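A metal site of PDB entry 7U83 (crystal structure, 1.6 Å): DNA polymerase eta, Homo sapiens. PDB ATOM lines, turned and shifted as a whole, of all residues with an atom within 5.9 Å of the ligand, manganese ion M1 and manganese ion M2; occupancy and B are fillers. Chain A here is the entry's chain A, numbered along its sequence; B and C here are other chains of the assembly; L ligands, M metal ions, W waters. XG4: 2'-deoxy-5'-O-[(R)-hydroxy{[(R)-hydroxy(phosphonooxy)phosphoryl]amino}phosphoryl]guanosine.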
ATOM      1  N   ASP A  16      -5.487  22.973  17.686  1.00  0.00           N
ATOM      2  CA  ASP A  16      -6.303  23.443  18.817  1.00  0.00           C
ATOM      3  C   ASP A  16      -7.245  24.553  18.359  1.00  0.00           C
ATOM      4  O   ASP A  16      -6.784  25.538  17.808  1.00  0.00           O
ATOM      5  CB  ASP A  16      -5.415  23.949  19.941  1.00  0.00           C
ATOM      6  CG  ASP A  16      -6.211  24.342  21.145  1.00  0.00           C
ATOM      7  OD1 ASP A  16      -6.777  25.411  21.084  1.00  0.00           O
ATOM      8  OD2 ASP A  16      -6.244  23.537  22.058  1.00  0.00           O
ATOM      9  N   MET A  17      -8.529  24.371  18.638  1.00  0.00           N
ATOM     10  CA  MET A  17      -9.493  25.381  18.140  1.00  0.00           C
ATOM     11  C   MET A  17      -9.295  26.711  18.893  1.00  0.00           C
ATOM     12  O   MET A  17      -9.059  26.701  20.058  1.00  0.00           O
ATOM     13  CB  MET A  17     -10.927  24.857  18.315  1.00  0.00           C
ATOM     14  CG  MET A  17     -11.152  23.480  17.760  1.00  0.00           C
ATOM     15  SD  MET A  17     -10.724  23.382  16.004  1.00  0.00           S
ATOM     16  CE  MET A  17     -11.912  24.506  15.312  1.00  0.00           C
ATOM     17  N   ASP A  18      -9.392  27.819  18.178  1.00  0.00           N
ATOM     18  CA  ASP A  18      -9.259  29.117  18.852  1.00  0.00           C
ATOM     19  C   ASP A  18     -10.542  29.412  19.653  1.00  0.00           C
ATOM     20  O   ASP A  18     -11.603  29.221  19.091  1.00  0.00           O
ATOM     21  CB  ASP A  18      -9.022  30.198  17.812  1.00  0.00           C
ATOM     22  CG  ASP A  18      -7.751  30.020  16.997  1.00  0.00           C
ATOM     23  OD1 ASP A  18      -6.792  29.473  17.520  1.00  0.00           O
ATOM     24  OD2 ASP A  18      -7.751  30.462  15.852  1.00  0.00           O
ATOM     25  N   CYS A  19     -10.410  29.928  20.880  1.00  0.00           N
ATOM     26  CA  CYS A  19     -11.591  30.311  21.735  1.00  0.00           C
ATOM     27  C   CYS A  19     -12.792  29.451  21.342  1.00  0.00           C
ATOM     28  O   CYS A  19     -13.790  30.019  20.988  1.00  0.00           O
ATOM     29  CB  CYS A  19     -11.813  31.818  21.704  1.00  0.00           C
ATOM     30  SG  CYS A  19     -11.957  32.607  20.085  1.00  0.00           S
ATOM     31  N   PHE A  20     -12.707  28.136  21.579  1.00  0.00           N
ATOM     32  CA  PHE A  20     -13.625  27.206  20.917  1.00  0.00           C
ATOM     33  C   PHE A  20     -15.091  27.487  21.265  1.00  0.00           C
ATOM     34  O   PHE A  20     -15.927  27.644  20.350  1.00  0.00           O
ATOM     35  CB  PHE A  20     -13.260  25.761  21.244  1.00  0.00           C
ATOM     36  CG  PHE A  20     -14.119  24.739  20.532  1.00  0.00           C
ATOM     37  CD1 PHE A  20     -14.360  24.842  19.182  1.00  0.00           C
ATOM     38  CD2 PHE A  20     -14.686  23.680  21.220  1.00  0.00           C
ATOM     39  CE1 PHE A  20     -15.175  23.884  18.506  1.00  0.00           C
ATOM     40  CE2 PHE A  20     -15.484  22.738  20.578  1.00  0.00           C
ATOM     41  CZ  PHE A  20     -15.704  22.829  19.221  1.00  0.00           C
ATOM     42  N   PHE A  21     -15.448  27.507  22.558  1.00  0.00           N
ATOM     43  CA  PHE A  21     -16.871  27.677  22.856  1.00  0.00           C
ATOM     44  C   PHE A  21     -17.394  29.013  22.336  1.00  0.00           C
ATOM     45  O   PHE A  21     -18.560  29.126  21.926  1.00  0.00           O
ATOM     46  CB  PHE A  21     -17.192  27.578  24.349  1.00  0.00           C
ATOM     47  CG  PHE A  21     -17.061  26.195  24.962  1.00  0.00           C
ATOM     48  CD1 PHE A  21     -16.392  25.149  24.335  1.00  0.00           C
ATOM     49  CD2 PHE A  21     -17.636  25.951  26.214  1.00  0.00           C
ATOM     50  CE1 PHE A  21     -16.283  23.876  24.961  1.00  0.00           C
ATOM     51  CE2 PHE A  21     -17.532  24.683  26.829  1.00  0.00           C
ATOM     52  CZ  PHE A  21     -16.867  23.651  26.194  1.00  0.00           C
ATOM     53  N   VAL A  22     -16.538  30.062  22.355  1.00  0.00           N
ATOM     54  CA  VAL A  22     -16.935  31.328  21.773  1.00  0.00           C
ATOM     55  C   VAL A  22     -17.223  31.169  20.282  1.00  0.00           C
ATOM     56  O   VAL A  22     -18.220  31.684  19.779  1.00  0.00           O
ATOM     57  CB  VAL A  22     -15.857  32.391  22.025  1.00  0.00           C
ATOM     58  CG1 VAL A  22     -16.046  33.593  21.092  1.00  0.00           C
ATOM     59  CG2 VAL A  22     -15.871  32.828  23.485  1.00  0.00           C
ATOM     60  N   GLN A  41     -20.785  30.110  32.445  1.00  0.00           N
ATOM     61  CA  GLN A  41     -21.727  29.154  32.999  1.00  0.00           C
ATOM     62  C   GLN A  41     -22.421  29.763  34.207  1.00  0.00           C
ATOM     63  O   GLN A  41     -21.752  30.298  35.101  1.00  0.00           O
ATOM     64  CB  GLN A  41     -21.102  27.785  33.348  1.00  0.00           C
ATOM     65  CG  GLN A  41     -19.891  27.384  32.522  1.00  0.00           C
ATOM     66  CD  GLN A  41     -19.264  26.063  32.997  1.00  0.00           C
ATOM     67  OE1 GLN A  41     -19.592  24.992  32.472  1.00  0.00           O
ATOM     68  NE2 GLN A  41     -18.376  26.146  33.971  1.00  0.00           N
ATOM     69  N   ILE A  51     -15.598  30.808  30.918  1.00  0.00           N
ATOM     70  CA  ILE A  51     -14.776  29.659  30.552  1.00  0.00           C
ATOM     71  C   ILE A  51     -14.105  29.797  29.182  1.00  0.00           C
ATOM     72  O   ILE A  51     -13.220  28.984  28.874  1.00  0.00           O
ATOM     73  CB  ILE A  51     -15.563  28.331  30.620  1.00  0.00           C
ATOM     74  CG1 ILE A  51     -16.848  28.369  29.764  1.00  0.00           C
ATOM     75  CG2 ILE A  51     -15.837  27.944  32.067  1.00  0.00           C
ATOM     76  CD1 ILE A  51     -17.508  26.989  29.665  1.00  0.00           C
ATOM     77  N   ALA A  52     -14.424  30.830  28.393  1.00  0.00           N
ATOM     78  CA  ALA A  52     -13.841  31.003  27.066  1.00  0.00           C
ATOM     79  C   ALA A  52     -13.976  32.465  26.676  1.00  0.00           C
ATOM     80  O   ALA A  52     -14.998  33.081  27.005  1.00  0.00           O
ATOM     81  CB  ALA A  52     -14.531  30.114  26.025  1.00  0.00           C
ATOM     82  N   VAL A  53     -12.959  32.999  25.979  1.00  0.00           N
ATOM     83  CA  VAL A  53     -12.849  34.444  25.744  1.00  0.00           C
ATOM     84  C   VAL A  53     -12.359  34.718  24.323  1.00  0.00           C
ATOM     85  O   VAL A  53     -11.303  34.218  23.930  1.00  0.00           O
ATOM     86  CB  VAL A  53     -11.893  35.097  26.760  1.00  0.00           C
ATOM     87  CG1 VAL A  53     -11.908  36.595  26.604  1.00  0.00           C
ATOM     88  CG2 VAL A  53     -12.297  34.761  28.150  1.00  0.00           C
ATOM     89  N   TYR A  55     -10.559  36.710  21.240  1.00  0.00           N
ATOM     90  CA  TYR A  55      -9.290  37.441  21.276  1.00  0.00           C
ATOM     91  C   TYR A  55      -9.490  38.956  21.410  1.00  0.00           C
ATOM     92  O   TYR A  55      -8.682  39.648  22.070  1.00  0.00           O
ATOM     93  CB  TYR A  55      -8.470  37.056  20.038  1.00  0.00           C
ATOM     94  CG  TYR A  55      -7.822  35.708  20.291  1.00  0.00           C
ATOM     95  CD1 TYR A  55      -8.569  34.549  20.181  1.00  0.00           C
ATOM     96  CD2 TYR A  55      -6.505  35.599  20.715  1.00  0.00           C
ATOM     97  CE1 TYR A  55      -8.009  33.304  20.442  1.00  0.00           C
ATOM     98  CE2 TYR A  55      -5.938  34.376  20.975  1.00  0.00           C
ATOM     99  CZ  TYR A  55      -6.704  33.229  20.872  1.00  0.00           C
ATOM    100  OH  TYR A  55      -6.142  31.994  21.137  1.00  0.00           O
ATOM    101  N   ARG A  58      -9.896  39.418  25.073  1.00  0.00           N
ATOM    102  CA  ARG A  58      -8.636  39.214  25.781  1.00  0.00           C
ATOM    103  C   ARG A  58      -7.789  40.474  25.770  1.00  0.00           C
ATOM    104  O   ARG A  58      -7.021  40.701  26.721  1.00  0.00           O
ATOM    105  CB  ARG A  58      -7.841  38.078  25.142  1.00  0.00           C
ATOM    106  CG  ARG A  58      -8.536  36.748  25.189  1.00  0.00           C
ATOM    107  CD  ARG A  58      -7.635  35.677  24.632  1.00  0.00           C
ATOM    108  NE  ARG A  58      -8.385  34.440  24.442  1.00  0.00           N
ATOM    109  CZ  ARG A  58      -7.845  33.254  24.224  1.00  0.00           C
ATOM    110  NH1 ARG A  58      -6.528  33.101  24.168  1.00  0.00           N
ATOM    111  NH2 ARG A  58      -8.635  32.185  24.102  1.00  0.00           N
ATOM    112  N   ARG A  64     -10.301  33.431  31.234  1.00  0.00           N
ATOM    113  CA  ARG A  64     -11.061  32.315  31.843  1.00  0.00           C
ATOM    114  C   ARG A  64     -10.915  32.405  33.370  1.00  0.00           C
ATOM    115  O   ARG A  64      -9.919  32.968  33.830  1.00  0.00           O
ATOM    116  CB  ARG A  64     -10.541  31.000  31.234  1.00  0.00           C
ATOM    117  CG  ARG A  64      -9.639  30.162  32.115  1.00  0.00           C
ATOM    118  CD  ARG A  64      -9.384  28.778  31.551  1.00  0.00           C
ATOM    119  NE  ARG A  64      -9.999  27.733  32.348  1.00  0.00           N
ATOM    120  CZ  ARG A  64      -9.566  27.311  33.531  1.00  0.00           C
ATOM    121  NH1 ARG A  64      -8.478  27.831  34.079  1.00  0.00           N
ATOM    122  NH2 ARG A  64     -10.226  26.358  34.171  1.00  0.00           N
ATOM    123  N   LEU A  92     -23.153  20.664  28.304  1.00  0.00           N
ATOM    124  CA  LEU A  92     -22.189  21.068  27.292  1.00  0.00           C
ATOM    125  C   LEU A  92     -22.381  20.345  25.957  1.00  0.00           C
ATOM    126  O   LEU A  92     -21.441  20.285  25.141  1.00  0.00           O
ATOM    127  CB  LEU A  92     -20.769  20.872  27.829  1.00  0.00           C
ATOM    128  CG  LEU A  92     -20.499  21.498  29.199  1.00  0.00           C
ATOM    129  CD1 LEU A  92     -19.140  21.154  29.701  1.00  0.00           C
ATOM    130  CD2 LEU A  92     -20.692  23.009  29.112  1.00  0.00           C
ATOM    131  N   SER A 116      -8.598  16.655  24.006  1.00  0.00           N
ATOM    132  CA  SER A 116      -9.602  17.446  24.750  1.00  0.00           C
ATOM    133  C   SER A 116     -10.795  17.674  23.831  1.00  0.00           C
ATOM    134  O   SER A 116     -10.759  17.250  22.695  1.00  0.00           O
ATOM    135  CB  SER A 116      -9.037  18.769  25.196  1.00  0.00           C
ATOM    136  OG  SER A 116      -9.136  19.728  24.158  1.00  0.00           O
ATOM    137  N   ILE A 117     -11.765  18.398  24.335  1.00  0.00           N
ATOM    138  CA  ILE A 117     -12.946  18.773  23.509  1.00  0.00           C
ATOM    139  C   ILE A 117     -12.510  19.615  22.294  1.00  0.00           C
ATOM    140  O   ILE A 117     -13.230  19.621  21.332  1.00  0.00           O
ATOM    141  CB  ILE A 117     -13.958  19.550  24.380  1.00  0.00           C
ATOM    142  CG1 ILE A 117     -15.356  19.551  23.770  1.00  0.00           C
ATOM    143  CG2 ILE A 117     -13.498  20.969  24.692  1.00  0.00           C
ATOM    144  CD1 ILE A 117     -16.441  19.940  24.752  1.00  0.00           C
ATOM    145  N   ASP A 118     -11.365  20.270  22.371  1.00  0.00           N
ATOM    146  CA  ASP A 118     -11.061  21.154  21.208  1.00  0.00           C
ATOM    147  C   ASP A 118      -9.685  20.917  20.571  1.00  0.00           C
ATOM    148  O   ASP A 118      -9.261  21.744  19.770  1.00  0.00           O
ATOM    149  CB  ASP A 118     -11.299  22.613  21.567  1.00  0.00           C
ATOM    150  CG  ASP A 118     -10.063  23.298  22.054  1.00  0.00           C
ATOM    151  OD1 ASP A 118      -9.344  22.658  22.814  1.00  0.00           O
ATOM    152  OD2 ASP A 118      -9.861  24.420  21.613  1.00  0.00           O
ATOM    153  N   GLU A 119      -9.033  19.818  20.912  1.00  0.00           N
ATOM    154  CA  GLU A 119      -7.722  19.624  20.285  1.00  0.00           C
ATOM    155  C   GLU A 119      -7.385  18.163  20.075  1.00  0.00           C
ATOM    156  O   GLU A 119      -7.879  17.307  20.819  1.00  0.00           O
ATOM    157  CB  GLU A 119      -6.622  20.279  21.101  1.00  0.00           C
ATOM    158  CG  GLU A 119      -6.238  19.543  22.360  1.00  0.00           C
ATOM    159  CD  GLU A 119      -5.790  20.493  23.439  1.00  0.00           C
ATOM    160  OE1 GLU A 119      -6.651  21.140  24.050  1.00  0.00           O
ATOM    161  OE2 GLU A 119      -4.590  20.614  23.621  1.00  0.00           O
ATOM    162  N   LYS A 227       2.472  20.888  20.857  1.00  0.00           N
ATOM    163  CA  LYS A 227       1.548  21.663  21.683  1.00  0.00           C
ATOM    164  C   LYS A 227       2.112  23.053  21.982  1.00  0.00           C
ATOM    165  O   LYS A 227       1.419  24.089  21.829  1.00  0.00           O
ATOM    166  CB  LYS A 227       1.257  20.891  22.974  1.00  0.00           C
ATOM    167  CG  LYS A 227       0.399  21.648  24.009  1.00  0.00           C
ATOM    168  CD  LYS A 227      -1.011  21.925  23.455  1.00  0.00           C
ATOM    169  CE  LYS A 227      -1.877  22.667  24.504  1.00  0.00           C
ATOM    170  NZ  LYS A 227      -3.286  22.962  24.045  1.00  0.00           N
ATOM    171  N   LYS A 234      -1.004  32.207  18.201  1.00  0.00           N
ATOM    172  CA  LYS A 234      -2.455  32.161  18.224  1.00  0.00           C
ATOM    173  C   LYS A 234      -2.983  33.582  18.138  1.00  0.00           C
ATOM    174  O   LYS A 234      -2.374  34.514  18.662  1.00  0.00           O
ATOM    175  CB  LYS A 234      -2.974  31.479  19.499  1.00  0.00           C
ATOM    176  CG  LYS A 234      -3.192  29.972  19.386  1.00  0.00           C
ATOM    177  CD  LYS A 234      -4.178  29.487  20.420  1.00  0.00           C
ATOM    178  CE  LYS A 234      -4.344  27.980  20.393  1.00  0.00           C
ATOM    179  NZ  LYS A 234      -5.668  27.655  19.791  1.00  0.00           N
ATOM    180  N   PRO A 235      -4.122  33.790  17.467  1.00  0.00           N
ATOM    181  CA  PRO A 235      -5.008  32.830  16.808  1.00  0.00           C
ATOM    182  C   PRO A 235      -4.823  32.677  15.309  1.00  0.00           C
ATOM    183  O   PRO A 235      -4.185  33.512  14.647  1.00  0.00           O
ATOM    184  CB  PRO A 235      -6.401  33.431  17.080  1.00  0.00           C
ATOM    185  CG  PRO A 235      -6.120  34.922  16.913  1.00  0.00           C
ATOM    186  CD  PRO A 235      -4.726  35.132  17.518  1.00  0.00           C
ATOM    187  P    DT B   3     -14.084  31.524  44.502  1.00  0.00           P
ATOM    188  OP1  DT B   3     -13.386  31.471  45.797  1.00  0.00           O
ATOM    189  OP2  DT B   3     -13.873  32.671  43.594  1.00  0.00           O
ATOM    190  O5'  DT B   3     -13.754  30.167  43.742  1.00  0.00           O
ATOM    191  C5'  DT B   3     -13.525  30.149  42.323  1.00  0.00           C
ATOM    192  C4'  DT B   3     -14.833  29.958  41.590  1.00  0.00           C
ATOM    193  O4'  DT B   3     -14.607  30.159  40.170  1.00  0.00           O
ATOM    194  C3'  DT B   3     -15.444  28.563  41.727  1.00  0.00           C
ATOM    195  O3'  DT B   3     -16.870  28.621  41.668  1.00  0.00           O
ATOM    196  C2'  DT B   3     -14.960  27.877  40.472  1.00  0.00           C
ATOM    197  C1'  DT B   3     -15.078  29.010  39.478  1.00  0.00           C
ATOM    198  N1   DT B   3     -14.212  28.802  38.323  1.00  0.00           N
ATOM    199  C2   DT B   3     -14.755  28.788  37.056  1.00  0.00           C
ATOM    200  O2   DT B   3     -15.940  29.006  36.837  1.00  0.00           O
ATOM    201  N3   DT B   3     -13.861  28.527  36.050  1.00  0.00           N
ATOM    202  C4   DT B   3     -12.511  28.264  36.175  1.00  0.00           C
ATOM    203  O4   DT B   3     -11.834  28.048  35.178  1.00  0.00           O
ATOM    204  C5   DT B   3     -12.015  28.285  37.537  1.00  0.00           C
ATOM    205  C7   DT B   3     -10.562  28.006  37.784  1.00  0.00           C
ATOM    206  C6   DT B   3     -12.873  28.536  38.519  1.00  0.00           C
ATOM    207  P    DT B   4     -17.738  27.305  41.921  1.00  0.00           P
ATOM    208  OP1  DT B   4     -19.084  27.723  42.356  1.00  0.00           O
ATOM    209  OP2  DT B   4     -16.945  26.382  42.745  1.00  0.00           O
ATOM    210  O5'  DT B   4     -17.830  26.632  40.483  1.00  0.00           O
ATOM    211  C5'  DT B   4     -18.459  27.278  39.371  1.00  0.00           C
ATOM    212  C4'  DT B   4     -18.507  26.332  38.190  1.00  0.00           C
ATOM    213  O4'  DT B   4     -17.263  26.377  37.466  1.00  0.00           O
ATOM    214  C3'  DT B   4     -18.730  24.859  38.562  1.00  0.00           C
ATOM    215  O3'  DT B   4     -19.836  24.455  37.753  1.00  0.00           O
ATOM    216  C2'  DT B   4     -17.407  24.197  38.234  1.00  0.00           C
ATOM    217  C1'  DT B   4     -16.851  25.068  37.129  1.00  0.00           C
ATOM    218  N1   DT B   4     -15.378  25.066  37.045  1.00  0.00           N
ATOM    219  C2   DT B   4     -14.778  25.070  35.807  1.00  0.00           C
ATOM    220  O2   DT B   4     -15.411  25.043  34.769  1.00  0.00           O
ATOM    221  N3   DT B   4     -13.414  25.094  35.834  1.00  0.00           N
ATOM    222  C4   DT B   4     -12.601  25.146  36.959  1.00  0.00           C
ATOM    223  O4   DT B   4     -11.383  25.121  36.827  1.00  0.00           O
ATOM    224  C5   DT B   4     -13.291  25.120  38.222  1.00  0.00           C
ATOM    225  C7   DT B   4     -12.491  25.112  39.480  1.00  0.00           C
ATOM    226  C6   DT B   4     -14.637  25.090  38.201  1.00  0.00           C
ATOM    227  P    DA B   5     -20.387  22.962  37.828  1.00  0.00           P
ATOM    228  OP1  DA B   5     -21.851  23.002  37.694  1.00  0.00           O
ATOM    229  OP2  DA B   5     -19.804  22.300  39.007  1.00  0.00           O
ATOM    230  O5'  DA B   5     -19.766  22.285  36.527  1.00  0.00           O
ATOM    231  C5'  DA B   5     -20.046  22.797  35.219  1.00  0.00           C
ATOM    232  C4'  DA B   5     -19.373  21.934  34.171  1.00  0.00           C
ATOM    233  O4'  DA B   5     -17.948  22.157  34.214  1.00  0.00           O
ATOM    234  C3'  DA B   5     -19.570  20.427  34.332  1.00  0.00           C
ATOM    235  O3'  DA B   5     -19.738  19.847  33.038  1.00  0.00           O
ATOM    236  C2'  DA B   5     -18.282  19.979  34.999  1.00  0.00           C
ATOM    237  C1'  DA B   5     -17.266  20.924  34.403  1.00  0.00           C
ATOM    238  N9   DA B   5     -16.130  21.175  35.278  1.00  0.00           N
ATOM    239  C8   DA B   5     -16.130  21.250  36.645  1.00  0.00           C
ATOM    240  N7   DA B   5     -14.952  21.496  37.168  1.00  0.00           N
ATOM    241  C5   DA B   5     -14.120  21.592  36.068  1.00  0.00           C
ATOM    242  C6   DA B   5     -12.740  21.834  35.944  1.00  0.00           C
ATOM    243  N6   DA B   5     -11.930  22.038  36.992  1.00  0.00           N
ATOM    244  N1   DA B   5     -12.215  21.869  34.699  1.00  0.00           N
ATOM    245  C2   DA B   5     -13.035  21.675  33.661  1.00  0.00           C
ATOM    246  N3   DA B   5     -14.335  21.425  33.647  1.00  0.00           N
ATOM    247  C4   DA B   5     -14.825  21.402  34.898  1.00  0.00           C
ATOM    248  P    DT C   8      -3.520  23.515  29.957  1.00  0.00           P
ATOM    249  OP1  DT C   8      -3.009  23.461  28.580  1.00  0.00           O
ATOM    250  OP2  DT C   8      -2.846  24.382  30.952  1.00  0.00           O
ATOM    251  O5'  DT C   8      -5.076  23.921  29.920  1.00  0.00           O
ATOM    252  C5'  DT C   8      -6.140  23.063  29.357  1.00  0.00           C
ATOM    253  C4'  DT C   8      -7.478  23.520  29.885  1.00  0.00           C
ATOM    254  O4'  DT C   8      -7.708  23.068  31.218  1.00  0.00           O
ATOM    255  C3'  DT C   8      -7.426  25.081  29.952  1.00  0.00           C
ATOM    256  O3'  DT C   8      -8.392  25.987  29.300  1.00  0.00           O
ATOM    257  C2'  DT C   8      -7.459  25.356  31.445  1.00  0.00           C
ATOM    258  C1'  DT C   8      -8.267  24.168  31.869  1.00  0.00           C
ATOM    259  N1   DT C   8      -8.305  23.864  33.275  1.00  0.00           N
ATOM    260  C2   DT C   8      -9.389  23.119  33.650  1.00  0.00           C
ATOM    261  O2   DT C   8     -10.207  22.703  32.847  1.00  0.00           O
ATOM    262  N3   DT C   8      -9.470  22.853  34.984  1.00  0.00           N
ATOM    263  C4   DT C   8      -8.598  23.262  35.972  1.00  0.00           C
ATOM    264  O4   DT C   8      -8.791  22.943  37.137  1.00  0.00           O
ATOM    265  C5   DT C   8      -7.476  24.052  35.514  1.00  0.00           C
ATOM    266  C7   DT C   8      -6.471  24.538  36.510  1.00  0.00           C
ATOM    267  C6   DT C   8      -7.390  24.319  34.205  1.00  0.00           C
HETATM  268  N1  XG4 L   1     -14.665  24.333  32.516  1.00  0.00           N
HETATM  269  C2  XG4 L   1     -15.392  24.044  31.386  1.00  0.00           C
HETATM  270  N2  XG4 L   1     -16.627  23.568  31.606  1.00  0.00           N
HETATM  271  N3  XG4 L   1     -15.005  24.213  30.128  1.00  0.00           N
HETATM  272  C4  XG4 L   1     -13.771  24.714  30.015  1.00  0.00           C
HETATM  273  C5  XG4 L   1     -12.948  25.034  31.036  1.00  0.00           C
HETATM  274  C6  XG4 L   1     -13.433  24.838  32.337  1.00  0.00           C
HETATM  275  O6  XG4 L   1     -12.765  25.134  33.337  1.00  0.00           O
HETATM  276  N7  XG4 L   1     -11.743  25.514  30.539  1.00  0.00           N
HETATM  277  C8  XG4 L   1     -11.879  25.479  29.232  1.00  0.00           C
HETATM  278  N9  XG4 L   1     -13.101  24.991  28.853  1.00  0.00           N
HETATM  279  PA  XG4 L   1      -8.893  25.795  25.462  1.00  0.00           P
HETATM  280  PB  XG4 L   1      -9.924  28.139  23.985  1.00  0.00           P
HETATM  281  PG  XG4 L   1      -7.483  29.187  22.862  1.00  0.00           P
HETATM  282  C1' XG4 L   1     -13.675  24.875  27.499  1.00  0.00           C
HETATM  283  O1A XG4 L   1      -8.286  25.244  24.239  1.00  0.00           O
HETATM  284  O1B XG4 L   1     -10.151  27.189  22.890  1.00  0.00           O
HETATM  285  O1G XG4 L   1      -6.472  29.888  23.780  1.00  0.00           O
HETATM  286  C2' XG4 L   1     -13.960  26.228  26.853  1.00  0.00           C
HETATM  287  O2A XG4 L   1      -7.919  25.709  26.708  1.00  0.00           O
HETATM  288  O2B XG4 L   1     -11.216  28.857  24.464  1.00  0.00           O
HETATM  289  O2G XG4 L   1      -7.230  27.691  22.675  1.00  0.00           O
HETATM  290  C3' XG4 L   1     -12.858  26.371  25.815  1.00  0.00           C
HETATM  291  O3' XG4 L   1     -13.372  27.101  24.705  1.00  0.00           O
HETATM  292  N3A XG4 L   1      -9.302  27.375  25.292  1.00  0.00           N
HETATM  293  O3B XG4 L   1      -8.905  29.270  23.557  1.00  0.00           O
HETATM  294  O3G XG4 L   1      -7.670  29.855  21.524  1.00  0.00           O
HETATM  295  C4' XG4 L   1     -12.556  24.926  25.440  1.00  0.00           C
HETATM  296  O4' XG4 L   1     -12.733  24.193  26.675  1.00  0.00           O
HETATM  297  C5' XG4 L   1     -11.178  24.667  24.886  1.00  0.00           C
HETATM  298  O5' XG4 L   1     -10.188  24.987  25.893  1.00  0.00           O
HETATM  299 MN    MN M   1      -7.514  23.139  23.855  1.00  0.00          MN
HETATM  300 MN    MN M   2      -8.519  26.073  22.054  1.00  0.00          MN
HETATM  301  O   HOH W   1      -8.370  22.376  25.845  1.00  0.00           O
HETATM  302  O   HOH W   2      -6.541  30.269  26.380  1.00  0.00           O
HETATM  303  O   HOH W   3      -5.844  24.154  25.052  1.00  0.00           O
HETATM  304  O   HOH W   4     -10.424  28.637  27.867  1.00  0.00           O
HETATM  305  O   HOH W   5     -10.838  31.222  25.719  1.00  0.00           O
HETATM  306  O   HOH W   6      -5.008  26.390  23.708  1.00  0.00           O
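An oxygen (O3G) of the ligand sits at hydrogen-bond distance from the side-chain hydroxyl (OH) of Tyr 55. O4' of DA 5 of chain B is in hydrogen-bond range of a nitrogen (N2) of the ligand (3.2 Å). The backbone NH (N) of Cys 19 sits at hydrogen-bond distance from an oxygen (O3G) of the ligand (2.8 Å). O2 of DT 4 of chain B lies within hydrogen-bond range of a nitrogen (N1) of the ligand. The side-chain amino group (NZ) of Lys 234 is in salt-bridge range of an oxygen (O3G) of the ligand (3.4 Å). O2B of the ligand sits at hydrogen-bond distance from N of Phe 20, at 3.3 Å. N3 of DA 5 of chain B is in hydrogen-bond range of a nitrogen (N1) of the ligand, at 3.1 Å. An oxygen (O6) of the ligand sits at hydrogen-bond distance from the guanidinium group of Arg 64 (2.9 Å). The side-chain amide oxygen (OE1) of Gln 41 is in hydrogen-bond range of a nitrogen (N2) of the ligand (3.4 Å). O3' of DT 8 of chain C lies close to O2A of the ligand, 2.6 Å away. The guanidinium group (NH2) of Arg 58 is in salt-bridge range of an oxygen (O1G) of the ligand (3.2 Å). An oxygen (O3') of the ligand is in hydrogen-bond range of the backbone NH (N) of Phe 21.
Manganese ion M1 is bound by the side-chain carboxylate (OD1) of Asp 118, the side-chain carboxylate (OE1) of Glu 119, the side-chain carboxylate (OD2) of Asp 16, an oxygen (O1A) of the ligand, water W3 and water W1. Manganese ion M1 has six donor atoms within binding distance.
Lys 234 touches manganese ion M2. Of the 26 residues printed, 4 come within 4 Å of manganese ion M2. The nearest printed residue that does not touch manganese ion M2 is Asp 18 (4.3 Å).
Manganese ion M2 is bound by OD1 of Asp 16. Manganese ion M2 is bound by an oxygen (O1B) of the ligand, 2.1 Å away. Manganese ion M2 is bound by O of Met 17 (2.2 Å). An oxygen (O2G) of the ligand is bound to manganese ion M2, at 2.2 Å. OD2 of Asp 118 is bound to manganese ion M2 (2.2 Å). O1A of the ligand binds manganese ion M2, at 2.3 Å.
Merely in contact with the ligand: Asp 18, Ile 51, Ala 52, Leu 92, Ile 117 and DT 3 of chain B. 20 residues have an atom within 4 Å of the ligand: Asp 16, Met 17, Asp 18, Cys 19, Phe 20, Phe 21, Gln 41, Ile 51, Ala 52, Tyr 55, Arg 58, Arg 64, Leu 92, Ile 117, Asp 118, Lys 234, DT 3 of chain B, DT 4 of chain B, DA 5 of chain B and DT 8 of chain C. The nearest printed residue that does not touch the ligand is Glu 119 (4.4 Å).
The guanidinium group of Arg 64 sits at hydrogen-bond distance from N1 of DT 8 of chain C, at 3.3 Å. The side-chain carboxylate (OD1) of Asp 18 lies within salt-bridge range of the side-chain amino group (NZ) of Lys 234, 3.1 Å away. O4 of DT 4 of chain B sits at hydrogen-bond distance from NH2 of Arg 64. The side-chain hydroxyl of Ser 116 is in hydrogen-bond range of the backbone NH of Glu 119 (3.2 Å). O2 of DT 4 of chain B is in hydrogen-bond range of the side-chain amide nitrogen of Gln 41. The side-chain carboxylate of Asp 16 lies close to the side-chain amino group of Lys 227 (3.6 Å). O of Asp 16 is in hydrogen-bond range of NZ of Lys 234 (3.1 Å). NH1 of Arg 58 is in hydrogen-bond range of OH of Tyr 55, at 3.2 Å.
Merely in contact with manganese ion M1: Ser 116 (3.8 Å). Four residues have an atom within 4 Å of manganese ion M1: Asp 16, Ser 116, Asp 118 and Glu 119.
Water W1 lies within hydrogen-bond range of O5' of the ligand (3.2 Å) and OG of Ser 116 (3.2 Å). Water W3 bridges the side-chain amino group of Lys 227 (3.0 Å) and an oxygen (O2A) of the ligand (3.1 Å). Water W5 lies within hydrogen-bond range of O2B of the ligand (2.7 Å), N of Val 53 (2.8 Å) and NH2 of Arg 58 (2.9 Å). Water W4 bridges O of Ile 51 (3.0 Å) and N3A of the ligand (3.1 Å).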
